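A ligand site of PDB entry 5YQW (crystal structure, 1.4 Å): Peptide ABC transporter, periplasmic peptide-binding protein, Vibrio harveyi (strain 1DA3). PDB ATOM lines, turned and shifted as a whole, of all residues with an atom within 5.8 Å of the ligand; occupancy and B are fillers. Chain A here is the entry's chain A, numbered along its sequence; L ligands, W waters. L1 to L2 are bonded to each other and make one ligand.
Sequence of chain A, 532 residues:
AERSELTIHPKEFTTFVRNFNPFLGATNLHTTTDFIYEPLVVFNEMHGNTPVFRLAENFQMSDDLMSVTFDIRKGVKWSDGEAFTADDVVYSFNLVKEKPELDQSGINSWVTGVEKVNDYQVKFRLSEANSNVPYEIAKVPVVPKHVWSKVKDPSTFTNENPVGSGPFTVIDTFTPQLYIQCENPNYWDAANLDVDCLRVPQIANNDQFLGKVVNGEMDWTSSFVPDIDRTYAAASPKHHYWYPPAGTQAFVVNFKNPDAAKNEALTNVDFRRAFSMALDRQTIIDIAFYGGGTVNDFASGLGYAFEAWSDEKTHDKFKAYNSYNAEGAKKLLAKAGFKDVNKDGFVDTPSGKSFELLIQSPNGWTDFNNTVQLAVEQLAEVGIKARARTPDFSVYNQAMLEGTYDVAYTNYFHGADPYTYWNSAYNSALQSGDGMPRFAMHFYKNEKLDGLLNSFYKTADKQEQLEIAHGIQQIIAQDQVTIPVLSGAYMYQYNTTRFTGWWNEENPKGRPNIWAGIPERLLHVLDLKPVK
The side-chain amide oxygen of Asn 206 sits at hydrogen-bond distance from an oxygen (O1) of LG2 L2, at 2.7 Å. OD1 of Asp 367 lies within hydrogen-bond range of O2 of LG2 L2. The side-chain amide nitrogen (ND2) of Asn 411 lies within hydrogen-bond range of an oxygen (O2) of LIG L1 (2.9 Å). The guanidinium group (NH2) of Arg 438 sits at hydrogen-bond distance from an oxygen (O6) of LIG L1. The indole nitrogen (NE1) of Trp 515 lies within hydrogen-bond range of an oxygen (O5) of LG2 L2 (2.9 Å). The backbone NH (N) of Phe 224 is in hydrogen-bond range of an oxygen (O1) of LG2 L2 (3.0 Å). The side-chain carboxylate of Glu 12 lies within hydrogen-bond range of an oxygen (O5) of LIG L1, 2.8 Å away. O5 of LG2 L2 is in hydrogen-bond range of OG of Ser 223 (3.4 Å).
OG1 of Thr 366 sits at hydrogen-bond distance from ND2 of Asn 206. The side-chain hydroxyl (OG) of Ser 222 sits close to the backbone carbonyl oxygen (O) of Met 491 (3.2 Å). The indole nitrogen (NE1) of Trp 515 sits close to the backbone carbonyl oxygen (O) of Ser 222 (3.3 Å). OD1 of Asn 411 sits at hydrogen-bond distance from NH2 of Arg 438. The backbone NH (N) of Phe 224 lies close to the side-chain sulfur (SD) of Met 491 (3.5 Å). The backbone carbonyl oxygen (O) of Gly 364 sits close to the backbone NH (N) of Asn 206 (3.2 Å). The side-chain hydroxyl (OG1) of Thr 410 sits at hydrogen-bond distance from the guanidinium group (NE) of Arg 438, at 2.9 Å.
An oxygen (O5) of LG2 L2 lies close to the backbone carbonyl oxygen of Ser 222. His 9 touches the ligand. Pro 10 touches the ligand. CD of Lys 11 touches O5 of LIG L1, 3.7 Å away. CA of Trp 365 touches O2 of LG2 L2 (3.3 Å). CE1 of Phe 368 touches O4 of LG2 L2 (3.5 Å). C of Tyr 412 touches C8 of LIG L1 (3.5 Å). N of Phe 413 touches C8 of LIG L1, at 3.7 Å. CZ of Phe 439 touches O6 of LIG L1, at 3.8 Å. CE of Met 491 touches O4 of LG2 L2, at 3.4 Å. Hydrophobic or aromatic side chains within 4 Å of the ligand: His 9, Phe 224, Trp 365, Phe 368, Phe 413, Phe 439, Met 491 and Trp 515.
Water W1 bridges O1 of LIG L1 (2.7 Å) and O of Ala 516 (2.7 Å). Water W6 lies within hydrogen-bond range of the backbone carbonyl oxygen of His 9 (2.8 Å), an oxygen (O5) of LG2 L2 (2.8 Å), the backbone NH of Ser 222 (2.8 Å) and the side-chain hydroxyl of Ser 223 (2.8 Å). Water W3 lies within hydrogen-bond range of a nitrogen (N1) of LIG L1 (2.8 Å) and the side-chain amide nitrogen (ND2) of Asn 411 (3.4 Å). Water W4 bridges an oxygen (O4) of LG2 L2 (2.8 Å) and the side-chain amide nitrogen (NE2) of Gln 249 (3.3 Å). Water W5 bridges O6 of LIG L1 and NH1 of Arg 438.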
ATOM      1  N   HIS A   9      -9.059 -12.744  16.894  1.00  0.00           N
ATOM      2  CA  HIS A   9      -9.409 -11.896  18.054  1.00  0.00           C
ATOM      3  C   HIS A   9      -9.165 -12.706  19.384  1.00  0.00           C
ATOM      4  O   HIS A   9     -10.092 -13.380  19.925  1.00  0.00           O
ATOM      5  CB  HIS A   9     -10.943 -11.458  17.957  1.00  0.00           C
ATOM      6  CG  HIS A   9     -11.388 -10.627  19.150  1.00  0.00           C
ATOM      7  ND1 HIS A   9     -10.557  -9.701  19.763  1.00  0.00           N
ATOM      8  CD2 HIS A   9     -12.596 -10.600  19.795  1.00  0.00           C
ATOM      9  CE1 HIS A   9     -11.245  -9.147  20.785  1.00  0.00           C
ATOM     10  NE2 HIS A   9     -12.488  -9.625  20.782  1.00  0.00           N
ATOM     11  N   PRO A  10      -7.908 -12.729  19.882  1.00  0.00           N
ATOM     12  CA  PRO A  10      -7.641 -13.618  21.078  1.00  0.00           C
ATOM     13  C   PRO A  10      -8.047 -12.961  22.403  1.00  0.00           C
ATOM     14  O   PRO A  10      -8.234 -13.679  23.387  1.00  0.00           O
ATOM     15  CB  PRO A  10      -6.119 -13.782  21.049  1.00  0.00           C
ATOM     16  CG  PRO A  10      -5.601 -12.643  20.189  1.00  0.00           C
ATOM     17  CD  PRO A  10      -6.674 -12.308  19.180  1.00  0.00           C
ATOM     18  N   LYS A  11      -8.187 -11.626  22.477  1.00  0.00           N
ATOM     19  CA  LYS A  11      -8.301 -10.926  23.807  1.00  0.00           C
ATOM     20  C   LYS A  11      -8.906  -9.532  23.578  1.00  0.00           C
ATOM     21  O   LYS A  11      -8.449  -8.770  22.714  1.00  0.00           O
ATOM     22  CB  LYS A  11      -6.864 -10.803  24.431  1.00  0.00           C
ATOM     23  CG  LYS A  11      -6.827 -10.005  25.775  1.00  0.00           C
ATOM     24  CD  LYS A  11      -7.621 -10.671  26.821  1.00  0.00           C
ATOM     25  CE  LYS A  11      -7.465 -10.062  28.236  1.00  0.00           C
ATOM     26  NZ  LYS A  11      -6.404  -9.041  28.285  1.00  0.00           N
ATOM     27  N   GLU A  12      -9.926  -9.169  24.352  1.00  0.00           N
ATOM     28  CA  GLU A  12     -10.424  -7.803  24.282  1.00  0.00           C
ATOM     29  C   GLU A  12      -9.541  -6.779  24.975  1.00  0.00           C
ATOM     30  O   GLU A  12      -8.879  -7.049  26.027  1.00  0.00           O
ATOM     31  CB  GLU A  12     -11.899  -7.766  24.766  1.00  0.00           C
ATOM     32  CG  GLU A  12     -12.250  -8.220  26.149  1.00  0.00           C
ATOM     33  CD  GLU A  12     -12.350  -9.760  26.178  1.00  0.00           C
ATOM     34  OE1 GLU A  12     -11.290 -10.321  26.490  1.00  0.00           O
ATOM     35  OE2 GLU A  12     -13.435 -10.383  25.925  1.00  0.00           O
ATOM     36  N   HIS A  30      -1.735 -10.953  23.211  1.00  0.00           N
ATOM     37  CA  HIS A  30      -2.041 -12.390  23.340  1.00  0.00           C
ATOM     38  C   HIS A  30      -1.840 -13.129  21.998  1.00  0.00           C
ATOM     39  O   HIS A  30      -2.420 -14.251  21.797  1.00  0.00           O
ATOM     40  CB  HIS A  30      -3.516 -12.571  23.801  1.00  0.00           C
ATOM     41  CG  HIS A  30      -3.680 -12.360  25.260  1.00  0.00           C
ATOM     42  ND1 HIS A  30      -4.535 -13.125  26.016  1.00  0.00           N
ATOM     43  CD2 HIS A  30      -3.056 -11.493  26.104  1.00  0.00           C
ATOM     44  CE1 HIS A  30      -4.472 -12.726  27.275  1.00  0.00           C
ATOM     45  NE2 HIS A  30      -3.577 -11.761  27.380  1.00  0.00           N
ATOM     46  N   ASN A 206     -18.242  -7.390  24.148  1.00  0.00           N
ATOM     47  CA  ASN A 206     -18.980  -8.296  23.313  1.00  0.00           C
ATOM     48  C   ASN A 206     -19.963  -7.532  22.435  1.00  0.00           C
ATOM     49  O   ASN A 206     -20.308  -8.087  21.348  1.00  0.00           O
ATOM     50  CB  ASN A 206     -19.760  -9.350  24.162  1.00  0.00           C
ATOM     51  CG  ASN A 206     -18.835 -10.435  24.764  1.00  0.00           C
ATOM     52  OD1 ASN A 206     -17.668 -10.524  24.414  1.00  0.00           O
ATOM     53  ND2 ASN A 206     -19.407 -11.196  25.722  1.00  0.00           N
ATOM     54  N   SER A 222     -13.440 -16.520  19.121  1.00  0.00           N
ATOM     55  CA  SER A 222     -13.888 -17.433  20.228  1.00  0.00           C
ATOM     56  C   SER A 222     -14.620 -16.576  21.306  1.00  0.00           C
ATOM     57  O   SER A 222     -14.523 -16.910  22.524  1.00  0.00           O
ATOM     58  CB  SER A 222     -12.694 -18.151  20.872  1.00  0.00           C
ATOM     59  OG  SER A 222     -11.997 -19.049  19.948  1.00  0.00           O
ATOM     60  N   SER A 223     -15.449 -15.610  20.868  1.00  0.00           N
ATOM     61  CA  SER A 223     -16.193 -14.802  21.804  1.00  0.00           C
ATOM     62  C   SER A 223     -17.624 -15.324  22.029  1.00  0.00           C
ATOM     63  O   SER A 223     -18.157 -16.130  21.294  1.00  0.00           O
ATOM     64  CB  SER A 223     -16.318 -13.354  21.202  1.00  0.00           C
ATOM     65  OG  SER A 223     -15.046 -12.684  21.242  1.00  0.00           O
ATOM     66  N   PHE A 224     -18.244 -14.872  23.160  1.00  0.00           N
ATOM     67  CA  PHE A 224     -19.643 -15.123  23.353  1.00  0.00           C
ATOM     68  C   PHE A 224     -20.480 -14.320  22.314  1.00  0.00           C
ATOM     69  O   PHE A 224     -20.254 -13.066  22.167  1.00  0.00           O
ATOM     70  CB  PHE A 224     -20.076 -14.697  24.801  1.00  0.00           C
ATOM     71  CG  PHE A 224     -21.546 -14.857  25.025  1.00  0.00           C
ATOM     72  CD1 PHE A 224     -22.151 -16.127  25.031  1.00  0.00           C
ATOM     73  CD2 PHE A 224     -22.360 -13.697  25.102  1.00  0.00           C
ATOM     74  CE1 PHE A 224     -23.549 -16.274  25.216  1.00  0.00           C
ATOM     75  CE2 PHE A 224     -23.815 -13.844  25.258  1.00  0.00           C
ATOM     76  CZ  PHE A 224     -24.382 -15.126  25.310  1.00  0.00           C
ATOM     77  N   GLN A 249     -17.397 -23.611  35.521  1.00  0.00           N
ATOM     78  CA  GLN A 249     -17.544 -22.180  35.921  1.00  0.00           C
ATOM     79  C   GLN A 249     -18.110 -22.178  37.348  1.00  0.00           C
ATOM     80  O   GLN A 249     -18.966 -23.016  37.678  1.00  0.00           O
ATOM     81  CB  GLN A 249     -18.511 -21.425  34.973  1.00  0.00           C
ATOM     82  CG  GLN A 249     -17.928 -21.387  33.559  1.00  0.00           C
ATOM     83  CD  GLN A 249     -18.751 -20.654  32.557  1.00  0.00           C
ATOM     84  OE1 GLN A 249     -19.671 -19.824  32.880  1.00  0.00           O
ATOM     85  NE2 GLN A 249     -18.355 -20.855  31.305  1.00  0.00           N
ATOM     86  N   PHE A 289     -26.752 -17.791  28.811  1.00  0.00           N
ATOM     87  CA  PHE A 289     -25.957 -18.468  27.765  1.00  0.00           C
ATOM     88  C   PHE A 289     -26.788 -18.965  26.586  1.00  0.00           C
ATOM     89  O   PHE A 289     -26.294 -19.750  25.760  1.00  0.00           O
ATOM     90  CB  PHE A 289     -25.142 -19.647  28.424  1.00  0.00           C
ATOM     91  CG  PHE A 289     -24.139 -19.172  29.442  1.00  0.00           C
ATOM     92  CD1 PHE A 289     -24.460 -19.010  30.854  1.00  0.00           C
ATOM     93  CD2 PHE A 289     -22.838 -18.952  29.024  1.00  0.00           C
ATOM     94  CE1 PHE A 289     -23.497 -18.548  31.759  1.00  0.00           C
ATOM     95  CE2 PHE A 289     -21.833 -18.518  29.956  1.00  0.00           C
ATOM     96  CZ  PHE A 289     -22.209 -18.293  31.340  1.00  0.00           C
ATOM     97  N   GLY A 364     -17.026  -6.336  29.846  1.00  0.00           N
ATOM     98  CA  GLY A 364     -17.209  -6.763  28.492  1.00  0.00           C
ATOM     99  C   GLY A 364     -17.573  -8.242  28.305  1.00  0.00           C
ATOM    100  O   GLY A 364     -18.054  -8.613  27.149  1.00  0.00           O
ATOM    101  N   TRP A 365     -17.441  -9.092  29.355  1.00  0.00           N
ATOM    102  CA  TRP A 365     -17.782 -10.551  29.243  1.00  0.00           C
ATOM    103  C   TRP A 365     -19.253 -10.652  29.635  1.00  0.00           C
ATOM    104  O   TRP A 365     -19.628 -11.062  30.754  1.00  0.00           O
ATOM    105  CB  TRP A 365     -16.901 -11.380  30.172  1.00  0.00           C
ATOM    106  CG  TRP A 365     -15.396 -11.343  30.019  1.00  0.00           C
ATOM    107  CD1 TRP A 365     -14.539 -10.352  29.423  1.00  0.00           C
ATOM    108  CD2 TRP A 365     -14.507 -12.410  30.465  1.00  0.00           C
ATOM    109  NE1 TRP A 365     -13.243 -10.775  29.510  1.00  0.00           N
ATOM    110  CE2 TRP A 365     -13.188 -11.995  30.134  1.00  0.00           C
ATOM    111  CE3 TRP A 365     -14.724 -13.628  31.220  1.00  0.00           C
ATOM    112  CZ2 TRP A 365     -12.041 -12.760  30.506  1.00  0.00           C
ATOM    113  CZ3 TRP A 365     -13.544 -14.425  31.490  1.00  0.00           C
ATOM    114  CH2 TRP A 365     -12.248 -13.933  31.186  1.00  0.00           C
ATOM    115  N   THR A 366     -20.111 -10.276  28.661  1.00  0.00           N
ATOM    116  CA  THR A 366     -21.551 -10.026  28.946  1.00  0.00           C
ATOM    117  C   THR A 366     -22.303 -11.291  29.458  1.00  0.00           C
ATOM    118  O   THR A 366     -23.269 -11.155  30.239  1.00  0.00           O
ATOM    119  CB  THR A 366     -22.331  -9.461  27.677  1.00  0.00           C
ATOM    120  OG1 THR A 366     -22.090 -10.372  26.575  1.00  0.00           O
ATOM    121  CG2 THR A 366     -21.847  -8.106  27.269  1.00  0.00           C
ATOM    122  N   ASP A 367     -21.941 -12.525  28.978  1.00  0.00           N
ATOM    123  CA  ASP A 367     -22.554 -13.774  29.457  1.00  0.00           C
ATOM    124  C   ASP A 367     -22.266 -13.878  31.001  1.00  0.00           C
ATOM    125  O   ASP A 367     -23.207 -14.234  31.760  1.00  0.00           O
ATOM    126  CB  ASP A 367     -22.068 -14.983  28.631  1.00  0.00           C
ATOM    127  CG  ASP A 367     -20.539 -15.022  28.451  1.00  0.00           C
ATOM    128  OD1 ASP A 367     -19.801 -14.076  28.647  1.00  0.00           O
ATOM    129  OD2 ASP A 367     -20.089 -16.176  28.112  1.00  0.00           O
ATOM    130  N   PHE A 368     -21.010 -13.632  31.417  1.00  0.00           N
ATOM    131  CA  PHE A 368     -20.685 -13.706  32.860  1.00  0.00           C
ATOM    132  C   PHE A 368     -21.347 -12.536  33.615  1.00  0.00           C
ATOM    133  O   PHE A 368     -21.809 -12.755  34.757  1.00  0.00           O
ATOM    134  CB  PHE A 368     -19.137 -13.657  33.008  1.00  0.00           C
ATOM    135  CG  PHE A 368     -18.465 -15.005  32.712  1.00  0.00           C
ATOM    136  CD1 PHE A 368     -18.992 -15.939  31.789  1.00  0.00           C
ATOM    137  CD2 PHE A 368     -17.185 -15.226  33.261  1.00  0.00           C
ATOM    138  CE1 PHE A 368     -18.255 -17.151  31.521  1.00  0.00           C
ATOM    139  CE2 PHE A 368     -16.486 -16.427  32.947  1.00  0.00           C
ATOM    140  CZ  PHE A 368     -17.006 -17.343  32.114  1.00  0.00           C
ATOM    141  N   PHE A 393     -10.657  -6.515  33.071  1.00  0.00           N
ATOM    142  CA  PHE A 393      -9.965  -7.784  33.403  1.00  0.00           C
ATOM    143  C   PHE A 393      -8.691  -7.627  34.208  1.00  0.00           C
ATOM    144  O   PHE A 393      -8.464  -8.395  35.174  1.00  0.00           O
ATOM    145  CB  PHE A 393      -9.712  -8.614  32.102  1.00  0.00           C
ATOM    146  CG  PHE A 393      -9.043  -9.945  32.410  1.00  0.00           C
ATOM    147  CD1 PHE A 393      -9.833 -11.057  32.693  1.00  0.00           C
ATOM    148  CD2 PHE A 393      -7.618 -10.008  32.518  1.00  0.00           C
ATOM    149  CE1 PHE A 393      -9.263 -12.280  33.072  1.00  0.00           C
ATOM    150  CE2 PHE A 393      -7.032 -11.231  32.868  1.00  0.00           C
ATOM    151  CZ  PHE A 393      -7.829 -12.330  33.199  1.00  0.00           C
ATOM    152  N   THR A 410     -15.946 -17.053  37.713  1.00  0.00           N
ATOM    153  CA  THR A 410     -14.780 -17.380  36.764  1.00  0.00           C
ATOM    154  C   THR A 410     -15.004 -18.745  36.125  1.00  0.00           C
ATOM    155  O   THR A 410     -15.680 -19.650  36.680  1.00  0.00           O
ATOM    156  CB  THR A 410     -13.393 -17.354  37.511  1.00  0.00           C
ATOM    157  OG1 THR A 410     -12.371 -17.516  36.541  1.00  0.00           O
ATOM    158  CG2 THR A 410     -13.219 -18.555  38.574  1.00  0.00           C
ATOM    159  N   ASN A 411     -14.410 -18.886  34.925  1.00  0.00           N
ATOM    160  CA  ASN A 411     -14.179 -20.234  34.383  1.00  0.00           C
ATOM    161  C   ASN A 411     -12.733 -20.676  34.683  1.00  0.00           C
ATOM    162  O   ASN A 411     -11.960 -19.998  35.351  1.00  0.00           O
ATOM    163  CB  ASN A 411     -14.449 -20.155  32.794  1.00  0.00           C
ATOM    164  CG  ASN A 411     -13.679 -19.023  32.094  1.00  0.00           C
ATOM    165  OD1 ASN A 411     -13.002 -18.210  32.667  1.00  0.00           O
ATOM    166  ND2 ASN A 411     -13.810 -19.025  30.755  1.00  0.00           N
ATOM    167  N   TYR A 412     -12.464 -21.859  34.170  1.00  0.00           N
ATOM    168  CA  TYR A 412     -11.124 -22.545  34.379  1.00  0.00           C
ATOM    169  C   TYR A 412     -10.761 -23.222  33.051  1.00  0.00           C
ATOM    170  O   TYR A 412     -11.640 -23.593  32.279  1.00  0.00           O
ATOM    171  CB  TYR A 412     -11.254 -23.687  35.494  1.00  0.00           C
ATOM    172  CG  TYR A 412     -11.702 -23.203  36.850  1.00  0.00           C
ATOM    173  CD1 TYR A 412     -13.123 -23.053  37.193  1.00  0.00           C
ATOM    174  CD2 TYR A 412     -10.767 -22.832  37.788  1.00  0.00           C
ATOM    175  CE1 TYR A 412     -13.472 -22.626  38.467  1.00  0.00           C
ATOM    176  CE2 TYR A 412     -11.135 -22.361  39.096  1.00  0.00           C
ATOM    177  CZ  TYR A 412     -12.504 -22.301  39.388  1.00  0.00           C
ATOM    178  OH  TYR A 412     -12.903 -21.989  40.702  1.00  0.00           O
ATOM    179  N   PHE A 413      -9.452 -23.470  32.889  1.00  0.00           N
ATOM    180  CA  PHE A 413      -8.968 -24.370  31.821  1.00  0.00           C
ATOM    181  C   PHE A 413      -9.491 -25.778  32.031  1.00  0.00           C
ATOM    182  O   PHE A 413      -9.822 -26.184  33.178  1.00  0.00           O
ATOM    183  CB  PHE A 413      -7.434 -24.236  31.755  1.00  0.00           C
ATOM    184  CG  PHE A 413      -7.024 -22.963  30.973  1.00  0.00           C
ATOM    185  CD1 PHE A 413      -7.213 -22.905  29.541  1.00  0.00           C
ATOM    186  CD2 PHE A 413      -6.663 -21.814  31.639  1.00  0.00           C
ATOM    187  CE1 PHE A 413      -6.916 -21.744  28.777  1.00  0.00           C
ATOM    188  CE2 PHE A 413      -6.272 -20.648  30.925  1.00  0.00           C
ATOM    189  CZ  PHE A 413      -6.460 -20.634  29.488  1.00  0.00           C
ATOM    190  N   ARG A 438      -5.353 -16.308  38.278  1.00  0.00           N
ATOM    191  CA  ARG A 438      -6.325 -16.070  39.370  1.00  0.00           C
ATOM    192  C   ARG A 438      -6.923 -17.323  39.944  1.00  0.00           C
ATOM    193  O   ARG A 438      -7.552 -17.237  40.997  1.00  0.00           O
ATOM    194  CB  ARG A 438      -7.494 -15.189  38.821  1.00  0.00           C
ATOM    195  CG  ARG A 438      -8.391 -16.043  37.822  1.00  0.00           C
ATOM    196  CD  ARG A 438      -9.302 -15.083  37.009  1.00  0.00           C
ATOM    197  NE  ARG A 438     -10.104 -15.782  36.012  1.00  0.00           N
ATOM    198  CZ  ARG A 438      -9.736 -15.988  34.703  1.00  0.00           C
ATOM    199  NH1 ARG A 438      -8.462 -15.647  34.316  1.00  0.00           N
ATOM    200  NH2 ARG A 438     -10.644 -16.551  33.894  1.00  0.00           N
ATOM    201  N   PHE A 439      -6.714 -18.528  39.349  1.00  0.00           N
ATOM    202  CA  PHE A 439      -7.708 -19.620  39.547  1.00  0.00           C
ATOM    203  C   PHE A 439      -7.680 -20.162  40.942  1.00  0.00           C
ATOM    204  O   PHE A 439      -8.748 -20.573  41.380  1.00  0.00           O
ATOM    205  CB  PHE A 439      -7.446 -20.754  38.523  1.00  0.00           C
ATOM    206  CG  PHE A 439      -7.493 -20.243  37.063  1.00  0.00           C
ATOM    207  CD1 PHE A 439      -8.754 -19.846  36.519  1.00  0.00           C
ATOM    208  CD2 PHE A 439      -6.314 -20.136  36.315  1.00  0.00           C
ATOM    209  CE1 PHE A 439      -8.820 -19.383  35.157  1.00  0.00           C
ATOM    210  CE2 PHE A 439      -6.368 -19.651  34.970  1.00  0.00           C
ATOM    211  CZ  PHE A 439      -7.616 -19.241  34.401  1.00  0.00           C
ATOM    212  N   MET A 491     -16.268 -21.721  22.878  1.00  0.00           N
ATOM    213  CA  MET A 491     -16.925 -20.876  21.837  1.00  0.00           C
ATOM    214  C   MET A 491     -15.971 -20.666  20.675  1.00  0.00           C
ATOM    215  O   MET A 491     -14.789 -20.224  20.911  1.00  0.00           O
ATOM    216  CB  MET A 491     -17.283 -19.497  22.444  1.00  0.00           C
ATOM    217  CG  MET A 491     -18.374 -19.506  23.511  1.00  0.00           C
ATOM    218  SD  MET A 491     -18.315 -18.071  24.635  1.00  0.00           S
ATOM    219  CE  MET A 491     -16.641 -18.229  25.271  1.00  0.00           C
ATOM    220  N   TRP A 515      -7.682 -18.319  21.727  1.00  0.00           N
ATOM    221  CA  TRP A 515      -7.115 -17.703  22.952  1.00  0.00           C
ATOM    222  C   TRP A 515      -5.659 -18.088  23.232  1.00  0.00           C
ATOM    223  O   TRP A 515      -5.244 -19.263  22.993  1.00  0.00           O
ATOM    224  CB  TRP A 515      -7.933 -18.159  24.139  1.00  0.00           C
ATOM    225  CG  TRP A 515      -9.443 -17.900  24.038  1.00  0.00           C
ATOM    226  CD1 TRP A 515     -10.115 -16.711  23.616  1.00  0.00           C
ATOM    227  CD2 TRP A 515     -10.485 -18.778  24.566  1.00  0.00           C
ATOM    228  NE1 TRP A 515     -11.498 -16.880  23.813  1.00  0.00           N
ATOM    229  CE2 TRP A 515     -11.733 -18.122  24.392  1.00  0.00           C
ATOM    230  CE3 TRP A 515     -10.451 -20.111  25.136  1.00  0.00           C
ATOM    231  CZ2 TRP A 515     -12.982 -18.692  24.786  1.00  0.00           C
ATOM    232  CZ3 TRP A 515     -11.712 -20.705  25.499  1.00  0.00           C
ATOM    233  CH2 TRP A 515     -12.973 -19.991  25.327  1.00  0.00           C
ATOM    234  N   ALA A 516      -4.966 -17.134  23.934  1.00  0.00           N
ATOM    235  CA  ALA A 516      -3.652 -17.572  24.508  1.00  0.00           C
ATOM    236  C   ALA A 516      -3.940 -18.704  25.606  1.00  0.00           C
ATOM    237  O   ALA A 516      -4.999 -18.706  26.316  1.00  0.00           O
ATOM    238  CB  ALA A 516      -2.979 -16.361  25.146  1.00  0.00           C
HETATM  239  C1  LIG L   1      -9.287 -16.845  28.194  1.00  0.00           C
HETATM  240  C2  LIG L   1     -10.581 -17.087  29.001  1.00  0.00           C
HETATM  241  C3  LIG L   1     -11.785 -16.907  27.983  1.00  0.00           C
HETATM  242  C4  LIG L   1     -11.679 -15.440  27.536  1.00  0.00           C
HETATM  243  C5  LIG L   1     -10.328 -15.221  26.893  1.00  0.00           C
HETATM  244  C6  LIG L   1     -10.171 -13.784  26.423  1.00  0.00           C
HETATM  245  C7  LIG L   1     -10.152 -18.812  30.823  1.00  0.00           C
HETATM  246  C8  LIG L   1     -10.270 -20.220  31.381  1.00  0.00           C
HETATM  247  N1  LIG L   1     -10.642 -18.507  29.532  1.00  0.00           N
HETATM  248  O1  LIG L   1      -8.172 -17.045  29.006  1.00  0.00           O
HETATM  249  O2  LIG L   1     -13.021 -17.120  28.711  1.00  0.00           O
HETATM  250  O3  LIG L   1     -12.663 -15.253  26.452  1.00  0.00           O
HETATM  251  O4  LIG L   1      -9.327 -15.404  27.962  1.00  0.00           O
HETATM  252  O5  LIG L   1     -10.487 -12.841  27.475  1.00  0.00           O
HETATM  253  O6  LIG L   1      -9.642 -17.913  31.515  1.00  0.00           O
HETATM  254  C1  LG2 L   2     -13.840 -14.493  26.791  1.00  0.00           C
HETATM  255  C2  LG2 L   2     -14.467 -13.973  25.473  1.00  0.00           C
HETATM  256  C3  LG2 L   2     -15.803 -13.228  25.823  1.00  0.00           C
HETATM  257  C4  LG2 L   2     -16.691 -14.088  26.687  1.00  0.00           C
HETATM  258  C5  LG2 L   2     -15.905 -14.501  27.929  1.00  0.00           C
HETATM  259  C6  LG2 L   2     -16.682 -15.479  28.834  1.00  0.00           C
HETATM  260  C7  LG2 L   2     -12.797 -13.313  23.683  1.00  0.00           C
HETATM  261  C8  LG2 L   2     -11.853 -12.190  23.218  1.00  0.00           C
HETATM  262  N1  LG2 L   2     -13.534 -13.044  24.790  1.00  0.00           N
HETATM  263  O1  LG2 L   2     -16.485 -12.946  24.559  1.00  0.00           O
HETATM  264  O2  LG2 L   2     -17.722 -13.171  27.158  1.00  0.00           O
HETATM  265  O3  LG2 L   2     -14.762 -15.331  27.468  1.00  0.00           O
HETATM  266  O4  LG2 L   2     -17.363 -16.564  28.183  1.00  0.00           O
HETATM  267  O5  LG2 L   2     -12.888 -14.419  23.139  1.00  0.00           O
HETATM  268  O   HOH W   1      -6.266 -16.478  27.250  1.00  0.00           O
HETATM  269  O   HOH W   2      -8.278 -12.904  29.531  1.00  0.00           O
HETATM  270  O   HOH W   3     -12.048 -20.643  28.368  1.00  0.00           O
HETATM  271  O   HOH W   4     -16.821 -19.246  28.856  1.00  0.00           O
HETATM  272  O   HOH W   5      -7.629 -15.900  31.577  1.00  0.00           O
HETATM  273  O   HOH W   6     -12.735 -14.084  20.378  1.00  0.00           O
